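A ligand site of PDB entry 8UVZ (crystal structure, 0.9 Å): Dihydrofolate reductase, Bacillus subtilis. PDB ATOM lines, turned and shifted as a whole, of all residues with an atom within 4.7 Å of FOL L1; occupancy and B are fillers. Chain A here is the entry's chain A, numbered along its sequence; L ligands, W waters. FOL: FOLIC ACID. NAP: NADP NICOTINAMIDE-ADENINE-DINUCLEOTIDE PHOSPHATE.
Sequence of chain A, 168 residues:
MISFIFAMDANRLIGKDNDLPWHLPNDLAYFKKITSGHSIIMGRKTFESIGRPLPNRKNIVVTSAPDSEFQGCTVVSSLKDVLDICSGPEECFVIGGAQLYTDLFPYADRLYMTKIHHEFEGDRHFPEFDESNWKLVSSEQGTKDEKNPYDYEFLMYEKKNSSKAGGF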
ATOM      1  N   ILE A   5      18.047  -7.388  -0.109  1.00  0.00           N
ATOM      2  CA  ILE A   5      17.028  -7.385  -1.158  1.00  0.00           C
ATOM      3  C   ILE A   5      16.605  -5.937  -1.332  1.00  0.00           C
ATOM      4  O   ILE A   5      16.474  -5.193  -0.348  1.00  0.00           O
ATOM      5  CB  ILE A   5      15.858  -8.333  -0.843  1.00  0.00           C
ATOM      6  CG1 ILE A   5      14.884  -8.359  -2.035  1.00  0.00           C
ATOM      7  CG2 ILE A   5      15.174  -7.983   0.459  1.00  0.00           C
ATOM      8  CD1 ILE A   5      13.950  -9.552  -2.013  1.00  0.00           C
ATOM      9  N   PHE A   6      16.443  -5.531  -2.587  1.00  0.00           N
ATOM     10  CA  PHE A   6      16.154  -4.151  -2.939  1.00  0.00           C
ATOM     11  C   PHE A   6      15.713  -4.104  -4.385  1.00  0.00           C
ATOM     12  O   PHE A   6      16.042  -4.991  -5.182  1.00  0.00           O
ATOM     13  CB  PHE A   6      17.356  -3.236  -2.734  1.00  0.00           C
ATOM     14  CG  PHE A   6      18.617  -3.662  -3.450  1.00  0.00           C
ATOM     15  CD1 PHE A   6      19.377  -4.713  -2.949  1.00  0.00           C
ATOM     16  CD2 PHE A   6      19.050  -3.029  -4.605  1.00  0.00           C
ATOM     17  CE1 PHE A   6      20.556  -5.115  -3.582  1.00  0.00           C
ATOM     18  CE2 PHE A   6      20.246  -3.426  -5.214  1.00  0.00           C
ATOM     19  CZ  PHE A   6      20.983  -4.455  -4.719  1.00  0.00           C
ATOM     20  N   ALA A   7      15.004  -3.036  -4.726  1.00  0.00           N
ATOM     21  CA  ALA A   7      14.684  -2.679  -6.093  1.00  0.00           C
ATOM     22  C   ALA A   7      15.234  -1.300  -6.373  1.00  0.00           C
ATOM     23  O   ALA A   7      15.021  -0.373  -5.577  1.00  0.00           O
ATOM     24  CB  ALA A   7      13.171  -2.687  -6.328  1.00  0.00           C
ATOM     25  N   LEU A  20       8.465   4.647  -1.871  1.00  0.00           N
ATOM     26  CA  LEU A  20       8.995   4.083  -3.087  1.00  0.00           C
ATOM     27  C   LEU A  20       8.681   5.022  -4.257  1.00  0.00           C
ATOM     28  O   LEU A  20       7.648   5.700  -4.253  1.00  0.00           O
ATOM     29  CB  LEU A  20       8.391   2.704  -3.367  1.00  0.00           C
ATOM     30  CG  LEU A  20       8.743   1.631  -2.335  1.00  0.00           C
ATOM     31  CD1 LEU A  20       7.944   0.350  -2.633  1.00  0.00           C
ATOM     32  CD2 LEU A  20      10.219   1.339  -2.284  1.00  0.00           C
ATOM     33  N   TRP A  22       7.812   4.218  -7.331  1.00  0.00           N
ATOM     34  CA  TRP A  22       7.044   3.535  -8.341  1.00  0.00           C
ATOM     35  C   TRP A  22       6.082   2.584  -7.670  1.00  0.00           C
ATOM     36  O   TRP A  22       6.109   2.407  -6.447  1.00  0.00           O
ATOM     37  CB  TRP A  22       8.003   2.734  -9.293  1.00  0.00           C
ATOM     38  CG  TRP A  22       8.881   1.801  -8.506  1.00  0.00           C
ATOM     39  CD1 TRP A  22       8.520   0.674  -7.859  1.00  0.00           C
ATOM     40  CD2 TRP A  22      10.266   2.014  -8.173  1.00  0.00           C
ATOM     41  NE1 TRP A  22       9.571   0.158  -7.131  1.00  0.00           N
ATOM     42  CE2 TRP A  22      10.654   0.982  -7.324  1.00  0.00           C
ATOM     43  CE3 TRP A  22      11.216   2.967  -8.581  1.00  0.00           C
ATOM     44  CZ2 TRP A  22      11.953   0.893  -6.801  1.00  0.00           C
ATOM     45  CZ3 TRP A  22      12.491   2.861  -8.079  1.00  0.00           C
ATOM     46  CH2 TRP A  22      12.853   1.846  -7.203  1.00  0.00           C
ATOM     47  N   PRO A  25       3.853  -4.205  -8.382  1.00  0.00           N
ATOM     48  CA  PRO A  25       3.316  -5.242  -7.489  1.00  0.00           C
ATOM     49  C   PRO A  25       3.969  -6.598  -7.645  1.00  0.00           C
ATOM     50  O   PRO A  25       4.082  -7.319  -6.648  1.00  0.00           O
ATOM     51  CB  PRO A  25       1.817  -5.241  -7.834  1.00  0.00           C
ATOM     52  CG  PRO A  25       1.685  -4.523  -9.076  1.00  0.00           C
ATOM     53  CD  PRO A  25       2.795  -3.552  -9.186  1.00  0.00           C
ATOM     54  N   ASP A  27       7.062  -7.176  -8.166  1.00  0.00           N
ATOM     55  CA  ASP A  27       8.297  -7.099  -7.375  1.00  0.00           C
ATOM     56  C   ASP A  27       8.008  -7.214  -5.888  1.00  0.00           C
ATOM     57  O   ASP A  27       8.744  -7.888  -5.163  1.00  0.00           O
ATOM     58  CB  ASP A  27       9.036  -5.811  -7.734  1.00  0.00           C
ATOM     59  CG  ASP A  27      10.221  -5.562  -6.846  1.00  0.00           C
ATOM     60  OD1 ASP A  27      11.121  -6.414  -6.763  1.00  0.00           O
ATOM     61  OD2 ASP A  27      10.224  -4.486  -6.220  1.00  0.00           O
ATOM     62  N   LEU A  28       6.934  -6.592  -5.391  1.00  0.00           N
ATOM     63  CA  LEU A  28       6.603  -6.791  -3.987  1.00  0.00           C
ATOM     64  C   LEU A  28       6.229  -8.244  -3.704  1.00  0.00           C
ATOM     65  O   LEU A  28       6.561  -8.780  -2.641  1.00  0.00           O
ATOM     66  CB  LEU A  28       5.512  -5.827  -3.530  1.00  0.00           C
ATOM     67  CG  LEU A  28       5.907  -4.347  -3.485  1.00  0.00           C
ATOM     68  CD1 LEU A  28       4.750  -3.538  -2.967  1.00  0.00           C
ATOM     69  CD2 LEU A  28       7.171  -4.117  -2.667  1.00  0.00           C
ATOM     70  N   ALA A  29       5.551  -8.913  -4.654  1.00  0.00           N
ATOM     71  CA  ALA A  29       5.241 -10.327  -4.477  1.00  0.00           C
ATOM     72  C   ALA A  29       6.521 -11.159  -4.428  1.00  0.00           C
ATOM     73  O   ALA A  29       6.627 -12.123  -3.649  1.00  0.00           O
ATOM     74  CB  ALA A  29       4.336 -10.789  -5.608  1.00  0.00           C
ATOM     75  N   PHE A  31       9.476  -9.993  -3.410  1.00  0.00           N
ATOM     76  CA  PHE A  31      10.036  -9.703  -2.109  1.00  0.00           C
ATOM     77  C   PHE A  31       9.420 -10.597  -1.026  1.00  0.00           C
ATOM     78  O   PHE A  31      10.125 -11.140  -0.184  1.00  0.00           O
ATOM     79  CB  PHE A  31       9.807  -8.212  -1.809  1.00  0.00           C
ATOM     80  CG  PHE A  31      10.154  -7.796  -0.416  1.00  0.00           C
ATOM     81  CD1 PHE A  31       9.222  -7.987   0.607  1.00  0.00           C
ATOM     82  CD2 PHE A  31      11.370  -7.231  -0.089  1.00  0.00           C
ATOM     83  CE1 PHE A  31       9.514  -7.619   1.899  1.00  0.00           C
ATOM     84  CE2 PHE A  31      11.635  -6.871   1.233  1.00  0.00           C
ATOM     85  CZ  PHE A  31      10.709  -7.063   2.211  1.00  0.00           C
ATOM     86  N   LYS A  32       8.105 -10.750  -1.050  1.00  0.00           N
ATOM     87  CA  LYS A  32       7.448 -11.600  -0.073  1.00  0.00           C
ATOM     88  C   LYS A  32       7.936 -13.053  -0.204  1.00  0.00           C
ATOM     89  O   LYS A  32       8.238 -13.716   0.805  1.00  0.00           O
ATOM     90  CB  LYS A  32       5.930 -11.531  -0.232  1.00  0.00           C
ATOM     91  CG  LYS A  32       5.173 -12.454   0.695  1.00  0.00           C
ATOM     92  CD  LYS A  32       3.660 -12.288   0.525  1.00  0.00           C
ATOM     93  CE  LYS A  32       2.892 -13.393   1.145  1.00  0.00           C
ATOM     94  NZ  LYS A  32       1.436 -13.212   0.942  1.00  0.00           N
ATOM     95  N   THR A  46      12.577   3.082   7.004  1.00  0.00           N
ATOM     96  CA  THR A  46      11.997   2.033   6.165  1.00  0.00           C
ATOM     97  C   THR A  46      10.818   1.376   6.878  1.00  0.00           C
ATOM     98  O   THR A  46       9.780   1.158   6.249  1.00  0.00           O
ATOM     99  CB  THR A  46      13.072   1.036   5.735  1.00  0.00           C
ATOM    100  OG1 THR A  46      13.943   1.692   4.814  1.00  0.00           O
ATOM    101  CG2 THR A  46      12.477  -0.166   5.038  1.00  0.00           C
ATOM    102  N   SER A  49       7.981   3.644   6.474  1.00  0.00           N
ATOM    103  CA  SER A  49       7.527   3.694   5.095  1.00  0.00           C
ATOM    104  C   SER A  49       6.610   2.516   4.777  1.00  0.00           C
ATOM    105  O   SER A  49       5.711   2.620   3.936  1.00  0.00           O
ATOM    106  CB  SER A  49       8.714   3.743   4.121  1.00  0.00           C
ATOM    107  OG  SER A  49       9.388   2.501   3.936  1.00  0.00           O
ATOM    108  N   ILE A  50       6.892   1.368   5.396  1.00  0.00           N
ATOM    109  CA  ILE A  50       6.072   0.190   5.246  1.00  0.00           C
ATOM    110  C   ILE A  50       4.779   0.375   6.036  1.00  0.00           C
ATOM    111  O   ILE A  50       3.678   0.182   5.501  1.00  0.00           O
ATOM    112  CB  ILE A  50       6.870  -1.050   5.687  1.00  0.00           C
ATOM    113  CG1 ILE A  50       8.050  -1.282   4.738  1.00  0.00           C
ATOM    114  CG2 ILE A  50       5.978  -2.278   5.708  1.00  0.00           C
ATOM    115  CD1 ILE A  50       9.070  -2.287   5.240  1.00  0.00           C
ATOM    116  N   LEU A  54       5.653  -6.655   8.681  1.00  0.00           N
ATOM    117  CA  LEU A  54       5.323  -7.613   7.634  1.00  0.00           C
ATOM    118  C   LEU A  54       5.073  -8.999   8.250  1.00  0.00           C
ATOM    119  O   LEU A  54       5.827  -9.442   9.122  1.00  0.00           O
ATOM    120  CB  LEU A  54       6.425  -7.656   6.612  1.00  0.00           C
ATOM    121  CG  LEU A  54       6.577  -6.363   5.806  1.00  0.00           C
ATOM    122  CD1 LEU A  54       7.807  -6.377   4.969  1.00  0.00           C
ATOM    123  CD2 LEU A  54       5.321  -6.099   4.957  1.00  0.00           C
ATOM    124  N   PRO A  55       4.041  -9.698   7.774  1.00  0.00           N
ATOM    125  CA  PRO A  55       3.662 -10.974   8.402  1.00  0.00           C
ATOM    126  C   PRO A  55       4.682 -12.071   8.099  1.00  0.00           C
ATOM    127  O   PRO A  55       5.354 -12.044   7.078  1.00  0.00           O
ATOM    128  CB  PRO A  55       2.294 -11.292   7.758  1.00  0.00           C
ATOM    129  CG  PRO A  55       2.325 -10.555   6.462  1.00  0.00           C
ATOM    130  CD  PRO A  55       3.082  -9.283   6.732  1.00  0.00           C
ATOM    131  N   ARG A  57       7.486 -12.958   9.295  1.00  0.00           N
ATOM    132  CA  ARG A  57       8.893 -12.608   9.362  1.00  0.00           C
ATOM    133  C   ARG A  57       9.121 -11.945  10.703  1.00  0.00           C
ATOM    134  O   ARG A  57       8.264 -11.201  11.167  1.00  0.00           O
ATOM    135  CB  ARG A  57       9.264 -11.631   8.250  1.00  0.00           C
ATOM    136  CG  ARG A  57       9.581 -12.311   6.923  1.00  0.00           C
ATOM    137  CD  ARG A  57       9.122 -11.524   5.719  1.00  0.00           C
ATOM    138  NE  ARG A  57       7.667 -11.479   5.637  1.00  0.00           N
ATOM    139  CZ  ARG A  57       7.008 -10.887   4.658  1.00  0.00           C
ATOM    140  NH1 ARG A  57       7.646 -10.333   3.631  1.00  0.00           N
ATOM    141  NH2 ARG A  57       5.677 -10.818   4.708  1.00  0.00           N
ATOM    142  N   ILE A  95      16.610  -5.178   4.367  1.00  0.00           N
ATOM    143  CA  ILE A  95      15.569  -4.644   3.492  1.00  0.00           C
ATOM    144  C   ILE A  95      15.587  -3.125   3.485  1.00  0.00           C
ATOM    145  O   ILE A  95      14.592  -2.492   3.140  1.00  0.00           O
ATOM    146  CB  ILE A  95      14.184  -5.209   3.835  1.00  0.00           C
ATOM    147  CG1 ILE A  95      13.614  -4.641   5.152  1.00  0.00           C
ATOM    148  CG2 ILE A  95      14.201  -6.719   3.853  1.00  0.00           C
ATOM    149  CD1 ILE A  95      12.110  -4.693   5.188  1.00  0.00           C
ATOM    150  N   TYR A 101      21.765  -0.225   3.618  1.00  0.00           N
ATOM    151  CA  TYR A 101      22.382  -0.849   2.467  1.00  0.00           C
ATOM    152  C   TYR A 101      23.821  -0.380   2.340  1.00  0.00           C
ATOM    153  O   TYR A 101      24.719  -1.155   1.999  1.00  0.00           O
ATOM    154  CB  TYR A 101      21.624  -0.536   1.188  1.00  0.00           C
ATOM    155  CG  TYR A 101      20.257  -1.158   1.043  1.00  0.00           C
ATOM    156  CD1 TYR A 101      20.021  -2.497   1.305  1.00  0.00           C
ATOM    157  CD2 TYR A 101      19.212  -0.395   0.570  1.00  0.00           C
ATOM    158  CE1 TYR A 101      18.753  -3.046   1.124  1.00  0.00           C
ATOM    159  CE2 TYR A 101      17.956  -0.929   0.377  1.00  0.00           C
ATOM    160  CZ  TYR A 101      17.729  -2.248   0.640  1.00  0.00           C
ATOM    161  OH  TYR A 101      16.456  -2.705   0.466  1.00  0.00           O
ATOM    162  N   THR A 114      16.342  -6.121  -7.790  1.00  0.00           N
ATOM    163  CA  THR A 114      15.387  -5.903  -8.879  1.00  0.00           C
ATOM    164  C   THR A 114      15.846  -4.661  -9.595  1.00  0.00           C
ATOM    165  O   THR A 114      15.852  -3.580  -9.002  1.00  0.00           O
ATOM    166  CB  THR A 114      13.963  -5.754  -8.390  1.00  0.00           C
ATOM    167  OG1 THR A 114      13.629  -6.922  -7.657  1.00  0.00           O
ATOM    168  CG2 THR A 114      13.014  -5.549  -9.566  1.00  0.00           C
HETATM  169  N1  FOL L   1      12.925  -5.071  -2.217  1.00  0.00           N
HETATM  170  C2  FOL L   1      12.345  -5.103  -3.359  1.00  0.00           C
HETATM  171  NA2 FOL L   1      12.669  -6.049  -4.304  1.00  0.00           N
HETATM  172  N3  FOL L   1      11.353  -4.249  -3.766  1.00  0.00           N
HETATM  173  C4  FOL L   1      10.919  -3.223  -2.979  1.00  0.00           C
HETATM  174  O4  FOL L   1      10.077  -2.401  -3.382  1.00  0.00           O
HETATM  175  C4A FOL L   1      11.487  -3.204  -1.677  1.00  0.00           C
HETATM  176  N5  FOL L   1      10.966  -2.341  -0.759  1.00  0.00           N
HETATM  177  C6  FOL L   1      11.435  -2.424   0.458  1.00  0.00           C
HETATM  178  C7  FOL L   1      12.498  -3.280   0.747  1.00  0.00           C
HETATM  179  N8  FOL L   1      12.987  -4.156  -0.110  1.00  0.00           N
HETATM  180  C8A FOL L   1      12.467  -4.126  -1.352  1.00  0.00           C
HETATM  181  C9  FOL L   1      10.851  -1.509   1.505  1.00  0.00           C
HETATM  182  N10 FOL L   1       9.454  -1.210   1.271  1.00  0.00           N
HETATM  183  C11 FOL L   1       6.353  -4.029   1.333  1.00  0.00           C
HETATM  184  C12 FOL L   1       7.657  -4.440   1.542  1.00  0.00           C
HETATM  185  C13 FOL L   1       8.698  -3.526   1.529  1.00  0.00           C
HETATM  186  C14 FOL L   1       8.429  -2.187   1.283  1.00  0.00           C
HETATM  187  C15 FOL L   1       7.133  -1.779   1.077  1.00  0.00           C
HETATM  188  C16 FOL L   1       6.095  -2.686   1.120  1.00  0.00           C
HETATM  189  C   FOL L   1       5.181  -4.977   1.389  1.00  0.00           C
HETATM  190  O   FOL L   1       4.040  -4.596   1.585  1.00  0.00           O
HETATM  191  N   FOL L   1       5.477  -6.312   1.200  1.00  0.00           N
HETATM  192  CA  FOL L   1       4.487  -7.359   1.304  1.00  0.00           C
HETATM  193  CB  FOL L   1       4.087  -7.639  -0.142  1.00  0.00           C
HETATM  194  CG  FOL L   1       2.950  -8.622  -0.212  1.00  0.00           C
HETATM  195  CD  FOL L   1       2.580  -8.736  -1.676  1.00  0.00           C
HETATM  196  OE1 FOL L   1       2.556  -7.715  -2.409  1.00  0.00           O
HETATM  197  OE2 FOL L   1       2.278  -9.840  -2.185  1.00  0.00           O
HETATM  198  CT  FOL L   1       5.148  -8.550   1.962  1.00  0.00           C
HETATM  199  O1  FOL L   1       4.415  -9.393   2.554  1.00  0.00           O
HETATM  200  O2  FOL L   1       6.362  -8.669   1.848  1.00  0.00           O
HETATM  201  PA  NAP L   2      16.554   4.035   6.814  1.00  0.00           P
HETATM  202  O1A NAP L   2      17.923   3.549   6.544  1.00  0.00           O
HETATM  203  O2A NAP L   2      15.430   3.089   6.583  1.00  0.00           O
HETATM  204  O5B NAP L   2      16.278   4.564   8.293  1.00  0.00           O
HETATM  205  C5B NAP L   2      17.241   5.464   8.888  1.00  0.00           C
HETATM  206  C4B NAP L   2      17.016   5.431  10.406  1.00  0.00           C
HETATM  207  O4B NAP L   2      17.308   4.060  10.849  1.00  0.00           O
HETATM  208  C3B NAP L   2      17.878   6.301  11.151  1.00  0.00           C
HETATM  209  O3B NAP L   2      17.363   7.623  11.278  1.00  0.00           O
HETATM  210  C2B NAP L   2      17.987   5.514  12.512  1.00  0.00           C
HETATM  211  O2B NAP L   2      16.736   5.583  13.234  1.00  0.00           O
HETATM  212  C1B NAP L   2      18.076   4.181  12.077  1.00  0.00           C
HETATM  213  N9A NAP L   2      19.439   3.733  11.695  1.00  0.00           N
HETATM  214  C8A NAP L   2      19.935   3.429  10.470  1.00  0.00           C
HETATM  215  N7A NAP L   2      21.166   2.981  10.523  1.00  0.00           N
HETATM  216  C5A NAP L   2      21.436   2.995  11.878  1.00  0.00           C
HETATM  217  C6A NAP L   2      22.524   2.601  12.576  1.00  0.00           C
HETATM  218  N6A NAP L   2      23.692   2.104  12.059  1.00  0.00           N
HETATM  219  N1A NAP L   2      22.467   2.695  13.924  1.00  0.00           N
HETATM  220  C2A NAP L   2      21.363   3.180  14.560  1.00  0.00           C
HETATM  221  N3A NAP L   2      20.263   3.562  13.935  1.00  0.00           N
HETATM  222  C4A NAP L   2      20.362   3.446  12.604  1.00  0.00           C
HETATM  223  O3  NAP L   2      16.278   5.383   6.017  1.00  0.00           O
HETATM  224  PN  NAP L   2      16.744   5.888   4.539  1.00  0.00           P
HETATM  225  O1N NAP L   2      18.180   5.650   4.231  1.00  0.00           O
HETATM  226  O2N NAP L   2      16.207   7.282   4.460  1.00  0.00           O
HETATM  227  O5D NAP L   2      15.903   4.930   3.578  1.00  0.00           O
HETATM  228  C5D NAP L   2      14.487   4.976   3.520  1.00  0.00           C
HETATM  229  C4D NAP L   2      13.972   5.165   2.108  1.00  0.00           C
HETATM  230  O4D NAP L   2      14.377   4.052   1.344  1.00  0.00           O
HETATM  231  C3D NAP L   2      12.370   5.262   1.810  1.00  0.00           C
HETATM  232  O3D NAP L   2      12.278   6.206   0.714  1.00  0.00           O
HETATM  233  C2D NAP L   2      12.039   3.966   1.456  1.00  0.00           C
HETATM  234  O2D NAP L   2      10.869   3.916   0.627  1.00  0.00           O
HETATM  235  C1D NAP L   2      13.238   3.495   0.637  1.00  0.00           C
HETATM  236  N1N NAP L   2      13.468   2.100   0.508  1.00  0.00           N
HETATM  237  C2N NAP L   2      13.457   1.531  -0.729  1.00  0.00           C
HETATM  238  C3N NAP L   2      13.743   0.190  -0.902  1.00  0.00           C
HETATM  239  C7N NAP L   2      13.846  -0.391  -2.283  1.00  0.00           C
HETATM  240  O7N NAP L   2      14.271  -1.512  -2.413  1.00  0.00           O
HETATM  241  N7N NAP L   2      13.477   0.356  -3.349  1.00  0.00           N
HETATM  242  C4N NAP L   2      14.024  -0.586   0.199  1.00  0.00           C
HETATM  243  C5N NAP L   2      13.964  -0.029   1.449  1.00  0.00           C
HETATM  244  C6N NAP L   2      13.706   1.319   1.618  1.00  0.00           C
HETATM  245  P2B NAP L   2      16.437   6.628  14.439  1.00  0.00           P
HETATM  246  O1X NAP L   2      16.483   7.999  13.782  1.00  0.00           O
HETATM  247  O2X NAP L   2      15.064   6.226  14.863  1.00  0.00           O
HETATM  248  O3X NAP L   2      17.487   6.397  15.483  1.00  0.00           O
HETATM  249  O   HOH W   1       0.860  -5.355  -1.459  1.00  0.00           O
HETATM  250  O   HOH W   2       1.980  -7.479  -4.916  1.00  0.00           O
HETATM  251  O   HOH W   3       8.743  -2.207  -5.686  1.00  0.00           O
HETATM  252  O   HOH W   4       9.260   1.798   1.318  1.00  0.00           O
HETATM  253  O   HOH W   5       1.969 -12.490  -3.182  1.00  0.00           O
HETATM  254  O   HOH W   6       1.873  -9.501   3.135  1.00  0.00           O
HETATM  255  O   HOH W   7      -0.155  -9.351   1.048  1.00  0.00           O
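O of Ala 7 is in hydrogen-bond range of N7N of NAP L2 (2.8 Å). An oxygen (O7N) of NAP L2 sits at hydrogen-bond distance from the backbone NH (N) of Ala 7 (2.9 Å). An oxygen (O2A) of NAP L2 sits at hydrogen-bond distance from the side-chain hydroxyl of Thr 46, 2.7 Å away. N3 of FOL L1 is in hydrogen-bond range of OD2 of Asp 27 (2.7 Å). An oxygen (O2) of FOL L1 lies within salt-bridge range of the guanidinium group (NH1) of Arg 57, 2.8 Å away. The backbone NH of Thr 46 is in hydrogen-bond range of an oxygen (O2A) of NAP L2, at 2.9 Å.
O of Ile 5 touches N8 of FOL L1 (3.6 Å). Phe 6 touches FOL L1 (CA to N1, 3.4 Å). Ala 7 touches FOL L1 (CB to N3, 3.5 Å). CD1 of Leu 20 touches O4 of FOL L1 (3.6 Å). Leu 28 touches FOL L1. CA of Ala 29 touches OE2 of FOL L1 (3.8 Å). Phe 31 touches FOL L1 (CD1 to O2, 3.2 Å). Lys 32 touches FOL L1 (CB to O2, 3.6 Å). CG1 of Ile 50 touches C14 of FOL L1, 3.6 Å away. Leu 54 touches FOL L1. Ile 95 touches FOL L1 (O to C7, 3.3 Å). Tyr 101 touches FOL L1. Thr 114 touches FOL L1 (OG1 to NA2, 3.6 Å). The nearest printed residue that does not touch FOL L1 is Thr 46 (4.1 Å).
The backbone carbonyl oxygen (O) of Ile 95 lies close to the side-chain hydroxyl (OH) of Tyr 101, 3.3 Å away. The backbone carbonyl oxygen (O) of Phe 6 sits at hydrogen-bond distance from the backbone NH (N) of Thr 114. O of Pro 55 lies within hydrogen-bond range of NH2 of Arg 57, at 2.7 Å. The backbone carbonyl oxygen of Ile 5 lies within hydrogen-bond range of the side-chain hydroxyl of Tyr 101 (2.6 Å). OD1 of Asp 27 is in hydrogen-bond range of OG1 of Thr 114 (2.7 Å).
Water W2 bridges OE1 of FOL L1 (2.6 Å) and O of Pro 25 (2.7 Å). Water W3 lies within hydrogen-bond range of an oxygen (O4) of FOL L1 (2.7 Å), the side-chain carboxylate of Asp 27 (2.8 Å) and the indole nitrogen of Trp 22 (2.9 Å). Water W4 lies within hydrogen-bond range of OG of Ser 49 (2.7 Å), O2D of NAP L2 (2.7 Å) and N10 of FOL L1 (3.0 Å).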
